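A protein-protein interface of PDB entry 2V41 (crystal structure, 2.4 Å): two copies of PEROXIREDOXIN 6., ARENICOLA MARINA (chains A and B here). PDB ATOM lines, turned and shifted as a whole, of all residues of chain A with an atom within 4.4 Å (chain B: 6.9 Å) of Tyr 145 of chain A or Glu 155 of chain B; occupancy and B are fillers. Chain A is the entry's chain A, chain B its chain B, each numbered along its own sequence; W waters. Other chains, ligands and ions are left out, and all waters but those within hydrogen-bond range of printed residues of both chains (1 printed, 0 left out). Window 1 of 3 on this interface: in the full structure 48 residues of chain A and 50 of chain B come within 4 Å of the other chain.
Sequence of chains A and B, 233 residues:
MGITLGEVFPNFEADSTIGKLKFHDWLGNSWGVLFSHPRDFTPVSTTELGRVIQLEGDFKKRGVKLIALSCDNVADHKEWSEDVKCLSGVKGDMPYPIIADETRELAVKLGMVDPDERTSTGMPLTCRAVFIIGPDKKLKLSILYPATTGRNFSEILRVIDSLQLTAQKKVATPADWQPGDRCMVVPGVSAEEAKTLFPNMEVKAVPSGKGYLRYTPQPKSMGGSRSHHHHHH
Of the printed residues of chain B, Leu 144 of chain A touches Leu 5 (3.9 Å), Leu 141 (3.5 Å) and Ser 142 (2.8 Å).
Printed residues of chain B within 4 Å of Tyr 145 of chain A: Leu 5 (3.99 Å), Leu 141 (3.6 Å), Glu 155 (2.6 Å) and Val 159 (3.6 Å).
Printed residues of chain B within 4 Å of Arg 151 of chain A: Arg 158.
Of the printed residues of chain A, Ser 142 of chain B touches Ile 143 and Leu 144.
Tyr 145 of chain B touches none of the printed residues of chain A.
Of the printed residues of chain A, Val 159 of chain B touches Tyr 145 (3.6 Å) and Thr 149 (3.9 Å).
Trp 177 of chain B touches none of the printed residues of chain A.
The nearest printed residue of chain B that does not touch Tyr 145 of chain A is Ile 143 of chain B (4.3 Å).
The nearest printed residue of chain A that does not touch Glu 155 of chain B is Arg 151 of chain A (5.2 Å).
Water W1 bridges O of Gly 150 of chain A (2.7 Å) and NH1 of Arg 158 of chain B (3.0 Å).
N of Leu 144 of chain A sits at hydrogen-bond distance from O of Ser 142 of chain B (2.8 Å).
OH of Tyr 145 of chain A lies within hydrogen-bond range of OE2 of Glu 155 of chain B, 2.6 Å away.
The backbone carbonyl oxygen of Gly 150 of chain A is in hydrogen-bond range of the guanidinium group of Arg 158 of chain B, at 3.1 Å.
ND2 of Asn 152 of chain A lies within hydrogen-bond range of OE1 of Glu 155 of chain B, 2.9 Å away.
Hydrophobic or aromatic side chains of chain B within 4 Å of the printed part of chain A: Leu 5, Leu 141, Val 159 and Leu 163.
Printed residues of chain A that touch a printed residue of chain B: Ile 143, Leu 144, Tyr 145, Pro 146, Thr 149, Gly 150, Arg 151 and Asn 152.
Among the printed residues, no Asp or Glu carboxylate lies within 4 Å of a Lys or Arg side-chain nitrogen of the other chain.
CA of Ile 143 of chain A touches O of Ser 142 of chain B, 3.7 Å away.
Leu 5 of chain B touches Leu 144 of chain A (CD1 to O, 3.9 Å).
Leu 144 of chain A touches Leu 141 of chain B (O to CA, 3.5 Å).
CE1 of Tyr 145 of chain A touches CD2 of Leu 141 of chain B, 3.6 Å away.
Tyr 145 of chain A touches Val 159 of chain B (CE2 to CG1, 3.6 Å).
CD1 of Leu 5 of chain B touches N of Pro 146 of chain A, 3.96 Å away.
O of Lys 140 of chain B touches CG of Pro 146 of chain A, at 3.6 Å.
Pro 146 of chain A touches Leu 163 of chain B (CG to CD2, 3.7 Å).
CG1 of Val 159 of chain B touches CG2 of Thr 149 of chain A, at 3.9 Å.
Arg 158 of chain B touches Asn 152 of chain A.
3 positions are printed for both chains.
The backbone carbonyl oxygen of Tyr 145 of chain A lies close to the side-chain sulfur of Cys 127 of chain A, 3.7 Å away.
N of Arg 128 of chain A sits at hydrogen-bond distance from O of Tyr 145 of chain A, at 2.9 Å.
The backbone carbonyl oxygen (O) of Ile 132 of chain B is in hydrogen-bond range of the backbone NH (N) of Lys 140 of chain B (2.7 Å).
OD1 of Asn 152 of chain B lies within hydrogen-bond range of N of Glu 155 of chain B (3.2 Å).
The side-chain carboxylate (OE1) of Glu 155 of chain B is in salt-bridge range of the guanidinium group (NE) of Arg 158 of chain B (2.9 Å).
The backbone carbonyl oxygen of Trp 177 of chain B is in hydrogen-bond range of the guanidinium group of Arg 158 of chain B (2.9 Å).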
ATOM      1  N   CYS A 127      -8.360   7.994  -0.770  1.00  0.00           N
ATOM      2  CA  CYS A 127      -7.590   6.916  -1.361  1.00  0.00           C
ATOM      3  C   CYS A 127      -8.602   5.824  -1.834  1.00  0.00           C
ATOM      4  O   CYS A 127      -9.816   6.096  -1.932  1.00  0.00           O
ATOM      5  CB  CYS A 127      -6.523   6.395  -0.362  1.00  0.00           C
ATOM      6  SG  CYS A 127      -7.209   5.685   1.175  1.00  0.00           S
ATOM      7  N   ARG A 128      -8.097   4.628  -2.156  1.00  0.00           N
ATOM      8  CA  ARG A 128      -8.906   3.448  -2.301  1.00  0.00           C
ATOM      9  C   ARG A 128      -8.975   2.671  -0.967  1.00  0.00           C
ATOM     10  O   ARG A 128      -8.183   1.783  -0.680  1.00  0.00           O
ATOM     11  CB  ARG A 128      -8.338   2.592  -3.418  1.00  0.00           C
ATOM     12  CG  ARG A 128      -8.060   3.376  -4.691  1.00  0.00           C
ATOM     13  CD  ARG A 128      -7.522   2.497  -5.827  1.00  0.00           C
ATOM     14  NE  ARG A 128      -7.069   3.397  -6.875  1.00  0.00           N
ATOM     15  CZ  ARG A 128      -7.868   4.081  -7.671  1.00  0.00           C
ATOM     16  NH1 ARG A 128      -9.178   3.893  -7.651  1.00  0.00           N
ATOM     17  NH2 ARG A 128      -7.341   4.949  -8.520  1.00  0.00           N
ATOM     18  N   ILE A 143      -8.997  -1.833   4.628  1.00  0.00           N
ATOM     19  CA  ILE A 143      -7.752  -1.668   3.836  1.00  0.00           C
ATOM     20  C   ILE A 143      -7.619  -0.213   3.363  1.00  0.00           C
ATOM     21  O   ILE A 143      -8.620   0.482   3.167  1.00  0.00           O
ATOM     22  CB  ILE A 143      -7.629  -2.667   2.655  1.00  0.00           C
ATOM     23  CG1 ILE A 143      -8.358  -2.142   1.447  1.00  0.00           C
ATOM     24  CG2 ILE A 143      -8.088  -4.044   3.037  1.00  0.00           C
ATOM     25  CD1 ILE A 143      -8.396  -3.052   0.220  1.00  0.00           C
ATOM     26  N   LEU A 144      -6.375   0.246   3.224  1.00  0.00           N
ATOM     27  CA  LEU A 144      -6.070   1.573   2.683  1.00  0.00           C
ATOM     28  C   LEU A 144      -5.030   1.413   1.561  1.00  0.00           C
ATOM     29  O   LEU A 144      -3.829   1.252   1.823  1.00  0.00           O
ATOM     30  CB  LEU A 144      -5.513   2.500   3.783  1.00  0.00           C
ATOM     31  CG  LEU A 144      -6.327   3.577   4.531  1.00  0.00           C
ATOM     32  CD1 LEU A 144      -7.733   3.339   4.607  1.00  0.00           C
ATOM     33  CD2 LEU A 144      -5.685   3.729   5.942  1.00  0.00           C
ATOM     34  N   TYR A 145      -5.512   1.475   0.333  1.00  0.00           N
ATOM     35  CA  TYR A 145      -4.694   1.416  -0.882  1.00  0.00           C
ATOM     36  C   TYR A 145      -4.631   2.818  -1.438  1.00  0.00           C
ATOM     37  O   TYR A 145      -5.586   3.503  -1.377  1.00  0.00           O
ATOM     38  CB  TYR A 145      -5.313   0.466  -1.943  1.00  0.00           C
ATOM     39  CG  TYR A 145      -5.083  -1.002  -1.697  1.00  0.00           C
ATOM     40  CD1 TYR A 145      -4.802  -1.503  -0.424  1.00  0.00           C
ATOM     41  CD2 TYR A 145      -5.176  -1.891  -2.717  1.00  0.00           C
ATOM     42  CE1 TYR A 145      -4.596  -2.835  -0.205  1.00  0.00           C
ATOM     43  CE2 TYR A 145      -4.986  -3.243  -2.502  1.00  0.00           C
ATOM     44  CZ  TYR A 145      -4.701  -3.699  -1.229  1.00  0.00           C
ATOM     45  OH  TYR A 145      -4.502  -5.055  -1.025  1.00  0.00           O
ATOM     46  N   PRO A 146      -3.513   3.218  -2.026  1.00  0.00           N
ATOM     47  CA  PRO A 146      -3.392   4.556  -2.607  1.00  0.00           C
ATOM     48  C   PRO A 146      -3.967   4.634  -4.020  1.00  0.00           C
ATOM     49  O   PRO A 146      -4.323   3.619  -4.625  1.00  0.00           O
ATOM     50  CB  PRO A 146      -1.890   4.765  -2.624  1.00  0.00           C
ATOM     51  CG  PRO A 146      -1.354   3.356  -2.892  1.00  0.00           C
ATOM     52  CD  PRO A 146      -2.259   2.434  -2.180  1.00  0.00           C
ATOM     53  N   ALA A 147      -4.050   5.845  -4.557  1.00  0.00           N
ATOM     54  CA  ALA A 147      -4.586   6.040  -5.865  1.00  0.00           C
ATOM     55  C   ALA A 147      -3.832   5.198  -6.889  1.00  0.00           C
ATOM     56  O   ALA A 147      -4.417   4.817  -7.942  1.00  0.00           O
ATOM     57  CB  ALA A 147      -4.530   7.493  -6.244  1.00  0.00           C
ATOM     58  N   THR A 149      -2.857   2.186  -6.918  1.00  0.00           N
ATOM     59  CA  THR A 149      -2.959   0.738  -6.750  1.00  0.00           C
ATOM     60  C   THR A 149      -4.387   0.240  -6.580  1.00  0.00           C
ATOM     61  O   THR A 149      -4.970   0.329  -5.492  1.00  0.00           O
ATOM     62  CB  THR A 149      -2.104   0.286  -5.587  1.00  0.00           C
ATOM     63  OG1 THR A 149      -0.770   0.723  -5.862  1.00  0.00           O
ATOM     64  CG2 THR A 149      -2.150  -1.269  -5.417  1.00  0.00           C
ATOM     65  N   GLY A 150      -4.934  -0.241  -7.696  1.00  0.00           N
ATOM     66  CA  GLY A 150      -6.267  -0.831  -7.731  1.00  0.00           C
ATOM     67  C   GLY A 150      -6.324  -2.048  -6.864  1.00  0.00           C
ATOM     68  O   GLY A 150      -5.363  -2.780  -6.751  1.00  0.00           O
ATOM     69  N   ARG A 151      -7.490  -2.247  -6.283  1.00  0.00           N
ATOM     70  CA  ARG A 151      -7.782  -3.310  -5.335  1.00  0.00           C
ATOM     71  C   ARG A 151      -8.133  -4.616  -6.030  1.00  0.00           C
ATOM     72  O   ARG A 151      -8.350  -4.669  -7.272  1.00  0.00           O
ATOM     73  CB  ARG A 151      -8.981  -2.889  -4.421  1.00  0.00           C
ATOM     74  CG  ARG A 151      -8.660  -1.797  -3.386  1.00  0.00           C
ATOM     75  CD  ARG A 151      -9.907  -1.020  -2.972  1.00  0.00           C
ATOM     76  NE  ARG A 151     -10.366  -0.120  -4.032  1.00  0.00           N
ATOM     77  CZ  ARG A 151     -11.254   0.857  -3.853  1.00  0.00           C
ATOM     78  NH1 ARG A 151     -11.802   1.069  -2.680  1.00  0.00           N
ATOM     79  NH2 ARG A 151     -11.611   1.635  -4.868  1.00  0.00           N
ATOM     80  N   ASN A 152      -8.134  -5.681  -5.202  1.00  0.00           N
ATOM     81  CA  ASN A 152      -8.403  -7.046  -5.633  1.00  0.00           C
ATOM     82  C   ASN A 152      -9.687  -7.409  -4.920  1.00  0.00           C
ATOM     83  O   ASN A 152      -9.680  -7.648  -3.719  1.00  0.00           O
ATOM     84  CB  ASN A 152      -7.266  -7.912  -5.179  1.00  0.00           C
ATOM     85  CG  ASN A 152      -7.533  -9.377  -5.363  1.00  0.00           C
ATOM     86  OD1 ASN A 152      -8.578  -9.734  -5.864  1.00  0.00           O
ATOM     87  ND2 ASN A 152      -6.581 -10.240  -4.937  1.00  0.00           N
ATOM     88  N   LEU B   5      -2.062   7.252   5.335  1.00  0.00           N
ATOM     89  CA  LEU B   5      -1.129   7.078   4.231  1.00  0.00           C
ATOM     90  C   LEU B   5      -0.402   8.394   3.994  1.00  0.00           C
ATOM     91  O   LEU B   5      -0.990   9.497   4.107  1.00  0.00           O
ATOM     92  CB  LEU B   5      -1.839   6.626   2.992  1.00  0.00           C
ATOM     93  CG  LEU B   5      -2.617   5.297   2.947  1.00  0.00           C
ATOM     94  CD1 LEU B   5      -2.990   4.996   1.471  1.00  0.00           C
ATOM     95  CD2 LEU B   5      -1.847   4.180   3.537  1.00  0.00           C
ATOM     96  N   ILE B 132       3.140  -1.189   4.662  1.00  0.00           N
ATOM     97  CA  ILE B 132       4.143  -1.118   3.593  1.00  0.00           C
ATOM     98  C   ILE B 132       4.744   0.315   3.552  1.00  0.00           C
ATOM     99  O   ILE B 132       4.021   1.343   3.314  1.00  0.00           O
ATOM    100  CB  ILE B 132       3.561  -1.519   2.242  1.00  0.00           C
ATOM    101  CG1 ILE B 132       2.892  -2.907   2.322  1.00  0.00           C
ATOM    102  CG2 ILE B 132       4.648  -1.500   1.150  1.00  0.00           C
ATOM    103  CD1 ILE B 132       2.366  -3.392   0.973  1.00  0.00           C
ATOM    104  N   LYS B 140       2.863   3.678   2.626  1.00  0.00           N
ATOM    105  CA  LYS B 140       2.369   3.673   1.254  1.00  0.00           C
ATOM    106  C   LYS B 140       1.057   2.887   1.119  1.00  0.00           C
ATOM    107  O   LYS B 140       0.300   3.120   0.241  1.00  0.00           O
ATOM    108  CB  LYS B 140       3.424   3.044   0.317  1.00  0.00           C
ATOM    109  CG  LYS B 140       4.760   3.708   0.210  1.00  0.00           C
ATOM    110  CD  LYS B 140       4.717   5.220   0.059  1.00  0.00           C
ATOM    111  CE  LYS B 140       5.896   5.821  -0.741  1.00  0.00           C
ATOM    112  NZ  LYS B 140       6.329   7.185  -0.199  1.00  0.00           N
ATOM    113  N   LEU B 141       0.837   1.916   1.977  1.00  0.00           N
ATOM    114  CA  LEU B 141      -0.313   1.028   1.920  1.00  0.00           C
ATOM    115  C   LEU B 141      -0.453   0.390   3.296  1.00  0.00           C
ATOM    116  O   LEU B 141       0.563   0.108   3.906  1.00  0.00           O
ATOM    117  CB  LEU B 141      -0.060  -0.081   0.907  1.00  0.00           C
ATOM    118  CG  LEU B 141      -1.214  -0.969   0.447  1.00  0.00           C
ATOM    119  CD1 LEU B 141      -1.121  -1.215  -1.087  1.00  0.00           C
ATOM    120  CD2 LEU B 141      -1.345  -2.279   1.279  1.00  0.00           C
ATOM    121  N   SER B 142      -1.690   0.156   3.763  1.00  0.00           N
ATOM    122  CA  SER B 142      -1.929  -0.599   5.018  1.00  0.00           C
ATOM    123  C   SER B 142      -3.190  -1.423   4.929  1.00  0.00           C
ATOM    124  O   SER B 142      -4.156  -1.060   4.249  1.00  0.00           O
ATOM    125  CB  SER B 142      -1.995   0.312   6.229  1.00  0.00           C
ATOM    126  OG  SER B 142      -3.192   1.054   6.216  1.00  0.00           O
ATOM    127  N   ILE B 143      -3.135  -2.592   5.552  1.00  0.00           N
ATOM    128  CA  ILE B 143      -4.313  -3.406   5.801  1.00  0.00           C
ATOM    129  C   ILE B 143      -4.419  -3.614   7.334  1.00  0.00           C
ATOM    130  O   ILE B 143      -3.422  -3.556   8.055  1.00  0.00           O
ATOM    131  CB  ILE B 143      -4.301  -4.763   4.993  1.00  0.00           C
ATOM    132  CG1 ILE B 143      -3.536  -5.860   5.696  1.00  0.00           C
ATOM    133  CG2 ILE B 143      -3.732  -4.590   3.581  1.00  0.00           C
ATOM    134  CD1 ILE B 143      -3.540  -7.196   4.977  1.00  0.00           C
ATOM    135  N   TYR B 145      -6.427  -6.472   9.298  1.00  0.00           N
ATOM    136  CA  TYR B 145      -7.232  -7.692   9.417  1.00  0.00           C
ATOM    137  C   TYR B 145      -7.348  -8.091  10.888  1.00  0.00           C
ATOM    138  O   TYR B 145      -6.430  -7.875  11.630  1.00  0.00           O
ATOM    139  CB  TYR B 145      -6.559  -8.860   8.640  1.00  0.00           C
ATOM    140  CG  TYR B 145      -6.708  -8.859   7.181  1.00  0.00           C
ATOM    141  CD1 TYR B 145      -6.921  -7.678   6.488  1.00  0.00           C
ATOM    142  CD2 TYR B 145      -6.591 -10.038   6.454  1.00  0.00           C
ATOM    143  CE1 TYR B 145      -7.028  -7.648   5.085  1.00  0.00           C
ATOM    144  CE2 TYR B 145      -6.729 -10.031   5.028  1.00  0.00           C
ATOM    145  CZ  TYR B 145      -6.945  -8.807   4.363  1.00  0.00           C
ATOM    146  OH  TYR B 145      -7.119  -8.684   2.988  1.00  0.00           O
ATOM    147  N   ASN B 152      -3.459 -12.730   3.112  1.00  0.00           N
ATOM    148  CA  ASN B 152      -3.139 -13.314   1.779  1.00  0.00           C
ATOM    149  C   ASN B 152      -1.839 -12.619   1.369  1.00  0.00           C
ATOM    150  O   ASN B 152      -1.863 -11.473   0.966  1.00  0.00           O
ATOM    151  CB  ASN B 152      -4.293 -12.980   0.826  1.00  0.00           C
ATOM    152  CG  ASN B 152      -4.060 -13.355  -0.622  1.00  0.00           C
ATOM    153  OD1 ASN B 152      -2.983 -13.689  -1.036  1.00  0.00           O
ATOM    154  ND2 ASN B 152      -5.107 -13.261  -1.400  1.00  0.00           N
ATOM    155  N   PHE B 153      -0.719 -13.335   1.501  1.00  0.00           N
ATOM    156  CA  PHE B 153       0.631 -12.852   1.155  1.00  0.00           C
ATOM    157  C   PHE B 153       0.948 -12.675  -0.354  1.00  0.00           C
ATOM    158  O   PHE B 153       1.878 -11.944  -0.709  1.00  0.00           O
ATOM    159  CB  PHE B 153       1.652 -13.723   1.901  1.00  0.00           C
ATOM    160  CG  PHE B 153       1.488 -13.595   3.378  1.00  0.00           C
ATOM    161  CD1 PHE B 153       0.566 -14.390   4.055  1.00  0.00           C
ATOM    162  CD2 PHE B 153       2.113 -12.569   4.051  1.00  0.00           C
ATOM    163  CE1 PHE B 153       0.333 -14.153   5.426  1.00  0.00           C
ATOM    164  CE2 PHE B 153       1.872 -12.324   5.383  1.00  0.00           C
ATOM    165  CZ  PHE B 153       0.986 -13.120   6.067  1.00  0.00           C
ATOM    166  N   SER B 154       0.143 -13.291  -1.215  1.00  0.00           N
ATOM    167  CA  SER B 154       0.237 -13.151  -2.670  1.00  0.00           C
ATOM    168  C   SER B 154      -0.222 -11.760  -3.063  1.00  0.00           C
ATOM    169  O   SER B 154       0.445 -11.060  -3.833  1.00  0.00           O
ATOM    170  CB  SER B 154      -0.634 -14.201  -3.375  1.00  0.00           C
ATOM    171  OG  SER B 154       0.003 -15.454  -3.267  1.00  0.00           O
ATOM    172  N   GLU B 155      -1.333 -11.354  -2.457  1.00  0.00           N
ATOM    173  CA  GLU B 155      -1.836  -9.992  -2.561  1.00  0.00           C
ATOM    174  C   GLU B 155      -0.856  -8.985  -2.021  1.00  0.00           C
ATOM    175  O   GLU B 155      -0.707  -7.949  -2.582  1.00  0.00           O
ATOM    176  CB  GLU B 155      -3.191  -9.864  -1.886  1.00  0.00           C
ATOM    177  CG  GLU B 155      -3.727  -8.448  -1.797  1.00  0.00           C
ATOM    178  CD  GLU B 155      -4.118  -7.851  -3.123  1.00  0.00           C
ATOM    179  OE1 GLU B 155      -4.361  -8.586  -4.095  1.00  0.00           O
ATOM    180  OE2 GLU B 155      -4.298  -6.632  -3.144  1.00  0.00           O
ATOM    181  N   ILE B 156      -0.153  -9.280  -0.962  1.00  0.00           N
ATOM    182  CA  ILE B 156       0.859  -8.338  -0.495  1.00  0.00           C
ATOM    183  C   ILE B 156       1.957  -8.158  -1.523  1.00  0.00           C
ATOM    184  O   ILE B 156       2.439  -7.105  -1.715  1.00  0.00           O
ATOM    185  CB  ILE B 156       1.385  -8.777   0.939  1.00  0.00           C
ATOM    186  CG1 ILE B 156       0.339  -8.379   2.013  1.00  0.00           C
ATOM    187  CG2 ILE B 156       2.732  -8.135   1.291  1.00  0.00           C
ATOM    188  CD1 ILE B 156       0.194  -9.350   3.204  1.00  0.00           C
ATOM    189  N   LEU B 157       2.330  -9.225  -2.222  1.00  0.00           N
ATOM    190  CA  LEU B 157       3.431  -9.176  -3.120  1.00  0.00           C
ATOM    191  C   LEU B 157       2.965  -8.429  -4.369  1.00  0.00           C
ATOM    192  O   LEU B 157       3.770  -7.854  -5.085  1.00  0.00           O
ATOM    193  CB  LEU B 157       3.952 -10.580  -3.445  1.00  0.00           C
ATOM    194  CG  LEU B 157       4.840 -11.292  -2.376  1.00  0.00           C
ATOM    195  CD1 LEU B 157       5.191 -12.676  -2.866  1.00  0.00           C
ATOM    196  CD2 LEU B 157       6.067 -10.577  -2.013  1.00  0.00           C
ATOM    197  N   ARG B 158       1.659  -8.492  -4.610  1.00  0.00           N
ATOM    198  CA  ARG B 158       1.038  -7.963  -5.788  1.00  0.00           C
ATOM    199  C   ARG B 158       1.053  -6.459  -5.679  1.00  0.00           C
ATOM    200  O   ARG B 158       1.523  -5.800  -6.557  1.00  0.00           O
ATOM    201  CB  ARG B 158      -0.380  -8.483  -5.921  1.00  0.00           C
ATOM    202  CG  ARG B 158      -0.999  -8.199  -7.307  1.00  0.00           C
ATOM    203  CD  ARG B 158      -2.522  -8.516  -7.352  1.00  0.00           C
ATOM    204  NE  ARG B 158      -3.258  -7.573  -6.537  1.00  0.00           N
ATOM    205  CZ  ARG B 158      -3.721  -6.373  -6.917  1.00  0.00           C
ATOM    206  NH1 ARG B 158      -3.604  -5.889  -8.156  1.00  0.00           N
ATOM    207  NH2 ARG B 158      -4.322  -5.635  -6.016  1.00  0.00           N
ATOM    208  N   VAL B 159       0.579  -5.930  -4.561  1.00  0.00           N
ATOM    209  CA  VAL B 159       0.539  -4.503  -4.333  1.00  0.00           C
ATOM    210  C   VAL B 159       1.924  -3.912  -4.164  1.00  0.00           C
ATOM    211  O   VAL B 159       2.115  -2.764  -4.456  1.00  0.00           O
ATOM    212  CB  VAL B 159      -0.353  -4.126  -3.126  1.00  0.00           C
ATOM    213  CG1 VAL B 159      -1.724  -4.607  -3.360  1.00  0.00           C
ATOM    214  CG2 VAL B 159       0.192  -4.659  -1.799  1.00  0.00           C
ATOM    215  N   ILE B 160       2.896  -4.691  -3.717  1.00  0.00           N
ATOM    216  CA  ILE B 160       4.330  -4.261  -3.787  1.00  0.00           C
ATOM    217  C   ILE B 160       4.826  -4.013  -5.218  1.00  0.00           C
ATOM    218  O   ILE B 160       5.548  -3.058  -5.500  1.00  0.00           O
ATOM    219  CB  ILE B 160       5.271  -5.283  -3.087  1.00  0.00           C
ATOM    220  CG1 ILE B 160       5.015  -5.240  -1.573  1.00  0.00           C
ATOM    221  CG2 ILE B 160       6.721  -4.928  -3.331  1.00  0.00           C
ATOM    222  CD1 ILE B 160       5.617  -6.295  -0.820  1.00  0.00           C
ATOM    223  N   LEU B 163       3.073  -0.729  -6.309  1.00  0.00           N
ATOM    224  CA  LEU B 163       3.722   0.419  -5.686  1.00  0.00           C
ATOM    225  C   LEU B 163       5.149   0.688  -6.202  1.00  0.00           C
ATOM    226  O   LEU B 163       5.572   1.850  -6.406  1.00  0.00           O
ATOM    227  CB  LEU B 163       3.787   0.211  -4.202  1.00  0.00           C
ATOM    228  CG  LEU B 163       2.512   0.075  -3.362  1.00  0.00           C
ATOM    229  CD1 LEU B 163       2.898  -0.600  -1.975  1.00  0.00           C
ATOM    230  CD2 LEU B 163       1.843   1.450  -3.205  1.00  0.00           C
ATOM    231  N   TRP B 177      -5.054  -6.291 -11.362  1.00  0.00           N
ATOM    232  CA  TRP B 177      -3.848  -6.336 -12.149  1.00  0.00           C
ATOM    233  C   TRP B 177      -2.857  -7.345 -11.594  1.00  0.00           C
ATOM    234  O   TRP B 177      -2.584  -7.356 -10.400  1.00  0.00           O
ATOM    235  CB  TRP B 177      -3.256  -4.919 -12.139  1.00  0.00           C
ATOM    236  CG  TRP B 177      -1.868  -4.785 -12.632  1.00  0.00           C
ATOM    237  CD1 TRP B 177      -1.483  -4.543 -13.885  1.00  0.00           C
ATOM    238  CD2 TRP B 177      -0.661  -4.840 -11.827  1.00  0.00           C
ATOM    239  NE1 TRP B 177      -0.093  -4.493 -13.951  1.00  0.00           N
ATOM    240  CE2 TRP B 177       0.424  -4.671 -12.695  1.00  0.00           C
ATOM    241  CE3 TRP B 177      -0.412  -5.037 -10.453  1.00  0.00           C
ATOM    242  CZ2 TRP B 177       1.733  -4.653 -12.257  1.00  0.00           C
ATOM    243  CZ3 TRP B 177       0.861  -5.063 -10.028  1.00  0.00           C
ATOM    244  CH2 TRP B 177       1.943  -4.874 -10.940  1.00  0.00           C
ATOM    245  N   GLN B 178      -2.304  -8.171 -12.473  1.00  0.00           N
ATOM    246  CA  GLN B 178      -1.118  -8.924 -12.178  1.00  0.00           C
ATOM    247  C   GLN B 178       0.054  -8.363 -12.971  1.00  0.00           C
ATOM    248  O   GLN B 178      -0.107  -7.910 -14.092  1.00  0.00           O
ATOM    249  CB  GLN B 178      -1.307 -10.399 -12.580  1.00  0.00           C
ATOM    250  CG  GLN B 178      -2.469 -11.133 -11.889  1.00  0.00           C
ATOM    251  CD  GLN B 178      -2.320 -11.151 -10.388  1.00  0.00           C
ATOM    252  OE1 GLN B 178      -3.286 -10.970  -9.685  1.00  0.00           O
ATOM    253  NE2 GLN B 178      -1.104 -11.310  -9.892  1.00  0.00           N
HETATM  254  O   HOH W   1      -3.768  -3.038  -8.967  1.00  0.00           O
